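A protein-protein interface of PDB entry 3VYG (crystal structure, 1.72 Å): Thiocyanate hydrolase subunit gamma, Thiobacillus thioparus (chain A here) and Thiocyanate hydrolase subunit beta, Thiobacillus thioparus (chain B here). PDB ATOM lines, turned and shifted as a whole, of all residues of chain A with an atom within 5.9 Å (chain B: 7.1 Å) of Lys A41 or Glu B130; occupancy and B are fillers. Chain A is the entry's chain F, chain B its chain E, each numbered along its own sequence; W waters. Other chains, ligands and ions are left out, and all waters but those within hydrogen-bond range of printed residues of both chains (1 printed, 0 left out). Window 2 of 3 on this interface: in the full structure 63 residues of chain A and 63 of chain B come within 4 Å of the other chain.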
ATOM      1  N   GLU A  36      -8.212  24.816 -21.521  1.00  0.00           N
ATOM      2  CA  GLU A  36      -7.727  24.539 -20.112  1.00  0.00           C
ATOM      3  C   GLU A  36      -6.247  24.558 -20.120  1.00  0.00           C
ATOM      4  O   GLU A  36      -5.653  25.248 -19.266  1.00  0.00           O
ATOM      5  CB  GLU A  36      -8.217  23.196 -19.596  1.00  0.00           C
ATOM      6  CG  GLU A  36      -9.709  23.332 -19.274  1.00  0.00           C
ATOM      7  CD  GLU A  36     -10.194  22.156 -18.400  1.00  0.00           C
ATOM      8  OE1 GLU A  36      -9.394  21.245 -18.116  1.00  0.00           O
ATOM      9  OE2 GLU A  36     -11.378  22.180 -17.995  1.00  0.00           O
ATOM     10  N   LEU A  37      -5.595  24.000 -21.143  1.00  0.00           N
ATOM     11  CA  LEU A  37      -4.110  24.102 -21.132  1.00  0.00           C
ATOM     12  C   LEU A  37      -3.597  25.565 -21.282  1.00  0.00           C
ATOM     13  O   LEU A  37      -2.619  25.949 -20.623  1.00  0.00           O
ATOM     14  CB  LEU A  37      -3.483  23.299 -22.314  1.00  0.00           C
ATOM     15  CG  LEU A  37      -3.577  21.785 -22.067  1.00  0.00           C
ATOM     16  CD1 LEU A  37      -3.406  21.037 -23.427  1.00  0.00           C
ATOM     17  CD2 LEU A  37      -2.490  21.329 -21.078  1.00  0.00           C
ATOM     18  N   ALA A  38      -4.200  26.382 -22.189  1.00  0.00           N
ATOM     19  CA  ALA A  38      -3.730  27.735 -22.365  1.00  0.00           C
ATOM     20  C   ALA A  38      -3.903  28.513 -21.029  1.00  0.00           C
ATOM     21  O   ALA A  38      -3.030  29.279 -20.660  1.00  0.00           O
ATOM     22  CB  ALA A  38      -4.590  28.470 -23.452  1.00  0.00           C
ATOM     23  N   ILE A  39      -5.026  28.297 -20.353  1.00  0.00           N
ATOM     24  CA  ILE A  39      -5.271  29.061 -19.078  1.00  0.00           C
ATOM     25  C   ILE A  39      -4.269  28.545 -18.017  1.00  0.00           C
ATOM     26  O   ILE A  39      -3.638  29.364 -17.297  1.00  0.00           O
ATOM     27  CB  ILE A  39      -6.711  28.866 -18.663  1.00  0.00           C
ATOM     28  CG1 ILE A  39      -7.566  29.688 -19.647  1.00  0.00           C
ATOM     29  CG2 ILE A  39      -6.855  29.343 -17.152  1.00  0.00           C
ATOM     30  CD1 ILE A  39      -9.108  29.356 -19.528  1.00  0.00           C
ATOM     31  N   GLU A  40      -4.056  27.222 -17.950  1.00  0.00           N
ATOM     32  CA  GLU A  40      -3.112  26.648 -16.947  1.00  0.00           C
ATOM     33  C   GLU A  40      -1.712  27.146 -17.197  1.00  0.00           C
ATOM     34  O   GLU A  40      -0.915  27.353 -16.215  1.00  0.00           O
ATOM     35  CB  GLU A  40      -3.123  25.087 -17.023  1.00  0.00           C
ATOM     36  CG  GLU A  40      -4.418  24.464 -16.583  1.00  0.00           C
ATOM     37  CD  GLU A  40      -4.556  22.973 -17.034  1.00  0.00           C
ATOM     38  OE1 GLU A  40      -5.611  22.385 -16.699  1.00  0.00           O
ATOM     39  OE2 GLU A  40      -3.676  22.397 -17.738  1.00  0.00           O
ATOM     40  N   LYS A  41      -1.313  27.354 -18.466  1.00  0.00           N
ATOM     41  CA  LYS A  41      -0.016  27.830 -18.702  1.00  0.00           C
ATOM     42  C   LYS A  41       0.118  29.348 -18.663  1.00  0.00           C
ATOM     43  O   LYS A  41       1.178  29.893 -18.980  1.00  0.00           O
ATOM     44  CB  LYS A  41       0.482  27.255 -20.099  1.00  0.00           C
ATOM     45  CG  LYS A  41       0.613  25.699 -20.107  1.00  0.00           C
ATOM     46  CD  LYS A  41       1.472  25.173 -18.974  1.00  0.00           C
ATOM     47  CE  LYS A  41       1.843  23.666 -19.297  1.00  0.00           C
ATOM     48  NZ  LYS A  41       2.822  23.197 -18.185  1.00  0.00           N
ATOM     49  N   GLY A  42      -0.999  30.051 -18.381  1.00  0.00           N
ATOM     50  CA  GLY A  42      -0.935  31.503 -18.272  1.00  0.00           C
ATOM     51  C   GLY A  42      -0.852  32.237 -19.578  1.00  0.00           C
ATOM     52  O   GLY A  42      -0.415  33.363 -19.608  1.00  0.00           O
ATOM     53  N   LEU A  43      -1.252  31.588 -20.660  1.00  0.00           N
ATOM     54  CA  LEU A  43      -1.112  32.231 -21.975  1.00  0.00           C
ATOM     55  C   LEU A  43      -2.213  33.287 -22.220  1.00  0.00           C
ATOM     56  O   LEU A  43      -1.907  34.395 -22.752  1.00  0.00           O
ATOM     57  CB  LEU A  43      -1.170  31.150 -23.030  1.00  0.00           C
ATOM     58  CG  LEU A  43      -0.141  30.045 -22.923  1.00  0.00           C
ATOM     59  CD1 LEU A  43      -0.169  29.061 -24.134  1.00  0.00           C
ATOM     60  CD2 LEU A  43       1.265  30.572 -22.869  1.00  0.00           C
ATOM     61  N   LEU B 120       0.471  25.786 -29.411  1.00  0.00           N
ATOM     62  CA  LEU B 120       0.903  25.506 -27.963  1.00  0.00           C
ATOM     63  C   LEU B 120       2.076  24.553 -27.966  1.00  0.00           C
ATOM     64  O   LEU B 120       2.988  24.726 -27.160  1.00  0.00           O
ATOM     65  CB  LEU B 120      -0.238  24.887 -27.170  1.00  0.00           C
ATOM     66  CG  LEU B 120      -1.418  25.814 -26.855  1.00  0.00           C
ATOM     67  CD1 LEU B 120      -2.453  25.105 -25.916  1.00  0.00           C
ATOM     68  CD2 LEU B 120      -1.263  27.272 -26.822  1.00  0.00           C
ATOM     69  N   GLN B 124       6.448  25.277 -27.681  1.00  0.00           N
ATOM     70  CA  GLN B 124       6.813  24.588 -26.375  1.00  0.00           C
ATOM     71  C   GLN B 124       6.103  25.146 -25.137  1.00  0.00           C
ATOM     72  O   GLN B 124       6.645  25.067 -24.035  1.00  0.00           O
ATOM     73  CB  GLN B 124       8.407  24.557 -26.243  1.00  0.00           C
ATOM     74  CG  GLN B 124       8.985  23.680 -27.307  1.00  0.00           C
ATOM     75  CD  GLN B 124      10.477  23.714 -27.402  1.00  0.00           C
ATOM     76  OE1 GLN B 124      11.041  24.645 -27.893  1.00  0.00           O
ATOM     77  NE2 GLN B 124      11.083  22.745 -26.858  1.00  0.00           N
ATOM     78  N   PHE B 125       4.933  25.770 -25.291  1.00  0.00           N
ATOM     79  CA  PHE B 125       4.188  26.188 -24.102  1.00  0.00           C
ATOM     80  C   PHE B 125       3.587  24.986 -23.386  1.00  0.00           C
ATOM     81  O   PHE B 125       3.356  25.007 -22.168  1.00  0.00           O
ATOM     82  CB  PHE B 125       3.090  27.181 -24.473  1.00  0.00           C
ATOM     83  CG  PHE B 125       3.658  28.495 -24.962  1.00  0.00           C
ATOM     84  CD1 PHE B 125       4.390  29.313 -24.077  1.00  0.00           C
ATOM     85  CD2 PHE B 125       3.509  28.894 -26.275  1.00  0.00           C
ATOM     86  CE1 PHE B 125       4.883  30.522 -24.552  1.00  0.00           C
ATOM     87  CE2 PHE B 125       3.956  30.087 -26.741  1.00  0.00           C
ATOM     88  CZ  PHE B 125       4.669  30.909 -25.851  1.00  0.00           C
ATOM     89  N   VAL B 126       3.362  23.934 -24.166  1.00  0.00           N
ATOM     90  CA  VAL B 126       2.796  22.677 -23.703  1.00  0.00           C
ATOM     91  C   VAL B 126       3.513  21.551 -24.440  1.00  0.00           C
ATOM     92  O   VAL B 126       3.678  21.617 -25.664  1.00  0.00           O
ATOM     93  CB  VAL B 126       1.283  22.692 -24.094  1.00  0.00           C
ATOM     94  CG1 VAL B 126       0.605  21.355 -23.923  1.00  0.00           C
ATOM     95  CG2 VAL B 126       0.516  23.835 -23.348  1.00  0.00           C
ATOM     96  N   THR B 127       3.960  20.524 -23.744  1.00  0.00           N
ATOM     97  CA  THR B 127       4.530  19.390 -24.410  1.00  0.00           C
ATOM     98  C   THR B 127       3.364  18.630 -25.157  1.00  0.00           C
ATOM     99  O   THR B 127       2.240  18.709 -24.772  1.00  0.00           O
ATOM    100  CB  THR B 127       5.274  18.398 -23.503  1.00  0.00           C
ATOM    101  OG1 THR B 127       4.360  17.738 -22.644  1.00  0.00           O
ATOM    102  CG2 THR B 127       6.296  19.163 -22.613  1.00  0.00           C
ATOM    103  N   LEU B 128       3.700  17.800 -26.129  1.00  0.00           N
ATOM    104  CA  LEU B 128       2.665  16.970 -26.824  1.00  0.00           C
ATOM    105  C   LEU B 128       2.128  15.974 -25.828  1.00  0.00           C
ATOM    106  O   LEU B 128       0.928  15.629 -25.801  1.00  0.00           O
ATOM    107  CB  LEU B 128       3.338  16.318 -28.059  1.00  0.00           C
ATOM    108  CG  LEU B 128       2.256  15.502 -28.785  1.00  0.00           C
ATOM    109  CD1 LEU B 128       1.221  16.544 -29.327  1.00  0.00           C
ATOM    110  CD2 LEU B 128       3.029  14.773 -29.915  1.00  0.00           C
ATOM    111  N   THR B 129       2.985  15.544 -24.909  1.00  0.00           N
ATOM    112  CA  THR B 129       2.565  14.653 -23.811  1.00  0.00           C
ATOM    113  C   THR B 129       1.494  15.342 -22.965  1.00  0.00           C
ATOM    114  O   THR B 129       0.471  14.739 -22.611  1.00  0.00           O
ATOM    115  CB  THR B 129       3.808  14.323 -22.910  1.00  0.00           C
ATOM    116  OG1 THR B 129       4.721  13.662 -23.753  1.00  0.00           O
ATOM    117  CG2 THR B 129       3.292  13.269 -21.849  1.00  0.00           C
ATOM    118  N   GLU B 130       1.713  16.593 -22.616  1.00  0.00           N
ATOM    119  CA  GLU B 130       0.615  17.283 -21.877  1.00  0.00           C
ATOM    120  C   GLU B 130      -0.667  17.388 -22.663  1.00  0.00           C
ATOM    121  O   GLU B 130      -1.739  17.157 -22.086  1.00  0.00           O
ATOM    122  CB  GLU B 130       1.053  18.675 -21.492  1.00  0.00           C
ATOM    123  CG  GLU B 130       2.142  18.626 -20.382  1.00  0.00           C
ATOM    124  CD  GLU B 130       2.751  19.988 -20.065  1.00  0.00           C
ATOM    125  OE1 GLU B 130       3.168  20.725 -20.965  1.00  0.00           O
ATOM    126  OE2 GLU B 130       2.835  20.391 -18.831  1.00  0.00           O
ATOM    127  N   LEU B 131      -0.551  17.606 -23.995  1.00  0.00           N
ATOM    128  CA  LEU B 131      -1.810  17.652 -24.764  1.00  0.00           C
ATOM    129  C   LEU B 131      -2.505  16.278 -24.866  1.00  0.00           C
ATOM    130  O   LEU B 131      -3.713  16.135 -24.638  1.00  0.00           O
ATOM    131  CB  LEU B 131      -1.486  18.257 -26.190  1.00  0.00           C
ATOM    132  CG  LEU B 131      -2.719  18.214 -27.146  1.00  0.00           C
ATOM    133  CD1 LEU B 131      -3.739  19.202 -26.634  1.00  0.00           C
ATOM    134  CD2 LEU B 131      -2.181  18.665 -28.453  1.00  0.00           C
ATOM    135  N   HIS B 132      -1.709  15.221 -25.159  1.00  0.00           N
ATOM    136  CA  HIS B 132      -2.302  13.887 -25.192  1.00  0.00           C
ATOM    137  C   HIS B 132      -2.886  13.484 -23.873  1.00  0.00           C
ATOM    138  O   HIS B 132      -4.009  12.989 -23.821  1.00  0.00           O
ATOM    139  CB  HIS B 132      -1.210  12.860 -25.583  1.00  0.00           C
ATOM    140  CG  HIS B 132      -0.746  12.933 -27.012  1.00  0.00           C
ATOM    141  ND1 HIS B 132       0.311  12.144 -27.429  1.00  0.00           N
ATOM    142  CD2 HIS B 132      -1.150  13.661 -28.077  1.00  0.00           C
ATOM    143  CE1 HIS B 132       0.527  12.362 -28.735  1.00  0.00           C
ATOM    144  NE2 HIS B 132      -0.365  13.270 -29.154  1.00  0.00           N
ATOM    145  N   ASN B 133      -2.199  13.837 -22.786  1.00  0.00           N
ATOM    146  CA  ASN B 133      -2.730  13.484 -21.487  1.00  0.00           C
ATOM    147  C   ASN B 133      -4.021  14.259 -21.216  1.00  0.00           C
ATOM    148  O   ASN B 133      -4.877  13.683 -20.566  1.00  0.00           O
ATOM    149  CB  ASN B 133      -1.791  13.843 -20.364  1.00  0.00           C
ATOM    150  CG  ASN B 133      -0.608  12.916 -20.256  1.00  0.00           C
ATOM    151  OD1 ASN B 133      -0.511  11.894 -20.928  1.00  0.00           O
ATOM    152  ND2 ASN B 133       0.372  13.335 -19.390  1.00  0.00           N
ATOM    153  N   LYS B 134      -4.096  15.532 -21.638  1.00  0.00           N
ATOM    154  CA  LYS B 134      -5.289  16.333 -21.322  1.00  0.00           C
ATOM    155  C   LYS B 134      -6.506  15.740 -22.093  1.00  0.00           C
ATOM    156  O   LYS B 134      -7.667  15.666 -21.578  1.00  0.00           O
ATOM    157  CB  LYS B 134      -4.991  17.770 -21.769  1.00  0.00           C
ATOM    158  CG  LYS B 134      -6.182  18.724 -21.595  1.00  0.00           C
ATOM    159  CD  LYS B 134      -6.524  18.975 -20.069  1.00  0.00           C
ATOM    160  CE  LYS B 134      -5.753  20.057 -19.425  1.00  0.00           C
ATOM    161  NZ  LYS B 134      -6.545  20.236 -18.093  1.00  0.00           N
ATOM    162  N   ILE B 135      -6.246  15.293 -23.336  1.00  0.00           N
ATOM    163  CA  ILE B 135      -7.324  14.666 -24.124  1.00  0.00           C
ATOM    164  C   ILE B 135      -7.833  13.372 -23.436  1.00  0.00           C
ATOM    165  O   ILE B 135      -9.033  13.145 -23.278  1.00  0.00           O
ATOM    166  CB  ILE B 135      -6.877  14.386 -25.574  1.00  0.00           C
ATOM    167  CG1 ILE B 135      -6.571  15.717 -26.294  1.00  0.00           C
ATOM    168  CG2 ILE B 135      -7.927  13.482 -26.290  1.00  0.00           C
ATOM    169  CD1 ILE B 135      -5.829  15.520 -27.653  1.00  0.00           C
ATOM    170  N   VAL B 136      -6.894  12.560 -22.970  1.00  0.00           N
ATOM    171  CA  VAL B 136      -7.247  11.364 -22.171  1.00  0.00           C
ATOM    172  C   VAL B 136      -8.149  11.757 -20.977  1.00  0.00           C
ATOM    173  O   VAL B 136      -9.225  11.169 -20.784  1.00  0.00           O
ATOM    174  CB  VAL B 136      -6.015  10.658 -21.576  1.00  0.00           C
ATOM    175  CG1 VAL B 136      -6.554   9.538 -20.607  1.00  0.00           C
ATOM    176  CG2 VAL B 136      -5.233   9.937 -22.711  1.00  0.00           C
HETATM  177  O   HOH W   1       5.230  22.246 -20.424  1.00  0.00           O
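Printed residues of chain B within 4 Å of Lys A41: Phe B125, Val B126 and Glu B130. Glu B130 touches one residue of chain A. Printed residues of chain A within 4 Å of Phe B125: Lys A41 and Leu A43. Of the printed residues of chain B, Glu A36 touches Lys B134 (3.0 Å). Of the printed residues of chain B, Glu A40 touches Lys B134. Printed residues of chain A within 4 Å of Leu B120: Leu A43 (3.4 Å). Of the printed residues of chain B, Leu A37 touches Leu B131 (3.7 Å) and Lys B134 (3.8 Å). Asn B133 touches none of the printed residues of chain A. The nearest printed residue of chain B that does not touch Lys A41 is Thr B127 (5.8 Å).
Of the 8 printed residues of chain A, 5 touch a printed residue of chain B. Printed residues of chain A that touch a printed residue of chain B: Glu A36, Leu A37, Glu A40, Lys A41 and Leu A43. Hydrophobic or aromatic side chains of chain A within 4 Å of the printed part of chain B: Leu A37 and Leu A43. Hydrophobic or aromatic side chains of chain B that line the printed part of chain A: Leu B120, Phe B125, Val B126 and Leu B131.
NZ of Lys A41 lies within salt-bridge range of OE2 of Glu B130 (2.9 Å). The side-chain carboxylate of Glu A36 is in salt-bridge range of the side-chain amino group of Lys B134 (3.0 Å). The side-chain carboxylate (OE1) of Glu A40 is in salt-bridge range of the side-chain amino group (NZ) of Lys B134 (2.7 Å).
Water W1 lies within hydrogen-bond range of OE1 of Glu B130 (2.6 Å) and NZ of Lys A41 (3.4 Å).
The backbone carbonyl oxygen of Leu B120 is in hydrogen-bond range of the backbone NH of Phe B125 (2.9 Å). O of Leu B120 lies within hydrogen-bond range of N of Val B126. OG1 of Thr B127 sits at hydrogen-bond distance from N of Glu B130, at 2.9 Å. The backbone carbonyl oxygen (O) of Ala A38 is in hydrogen-bond range of the backbone NH (N) of Leu A43.
Leu A37 touches Leu B131 (CD1 to CD1, 3.7 Å). Leu A37 touches Lys B134 (CG to CE, 3.8 Å). Lys A41 touches Phe B125 (CG to O, 3.5 Å). Lys A41 touches Val B126. Leu B120 touches Leu A43. CD2 of Leu A43 touches CD1 of Phe B125, 3.6 Å away.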
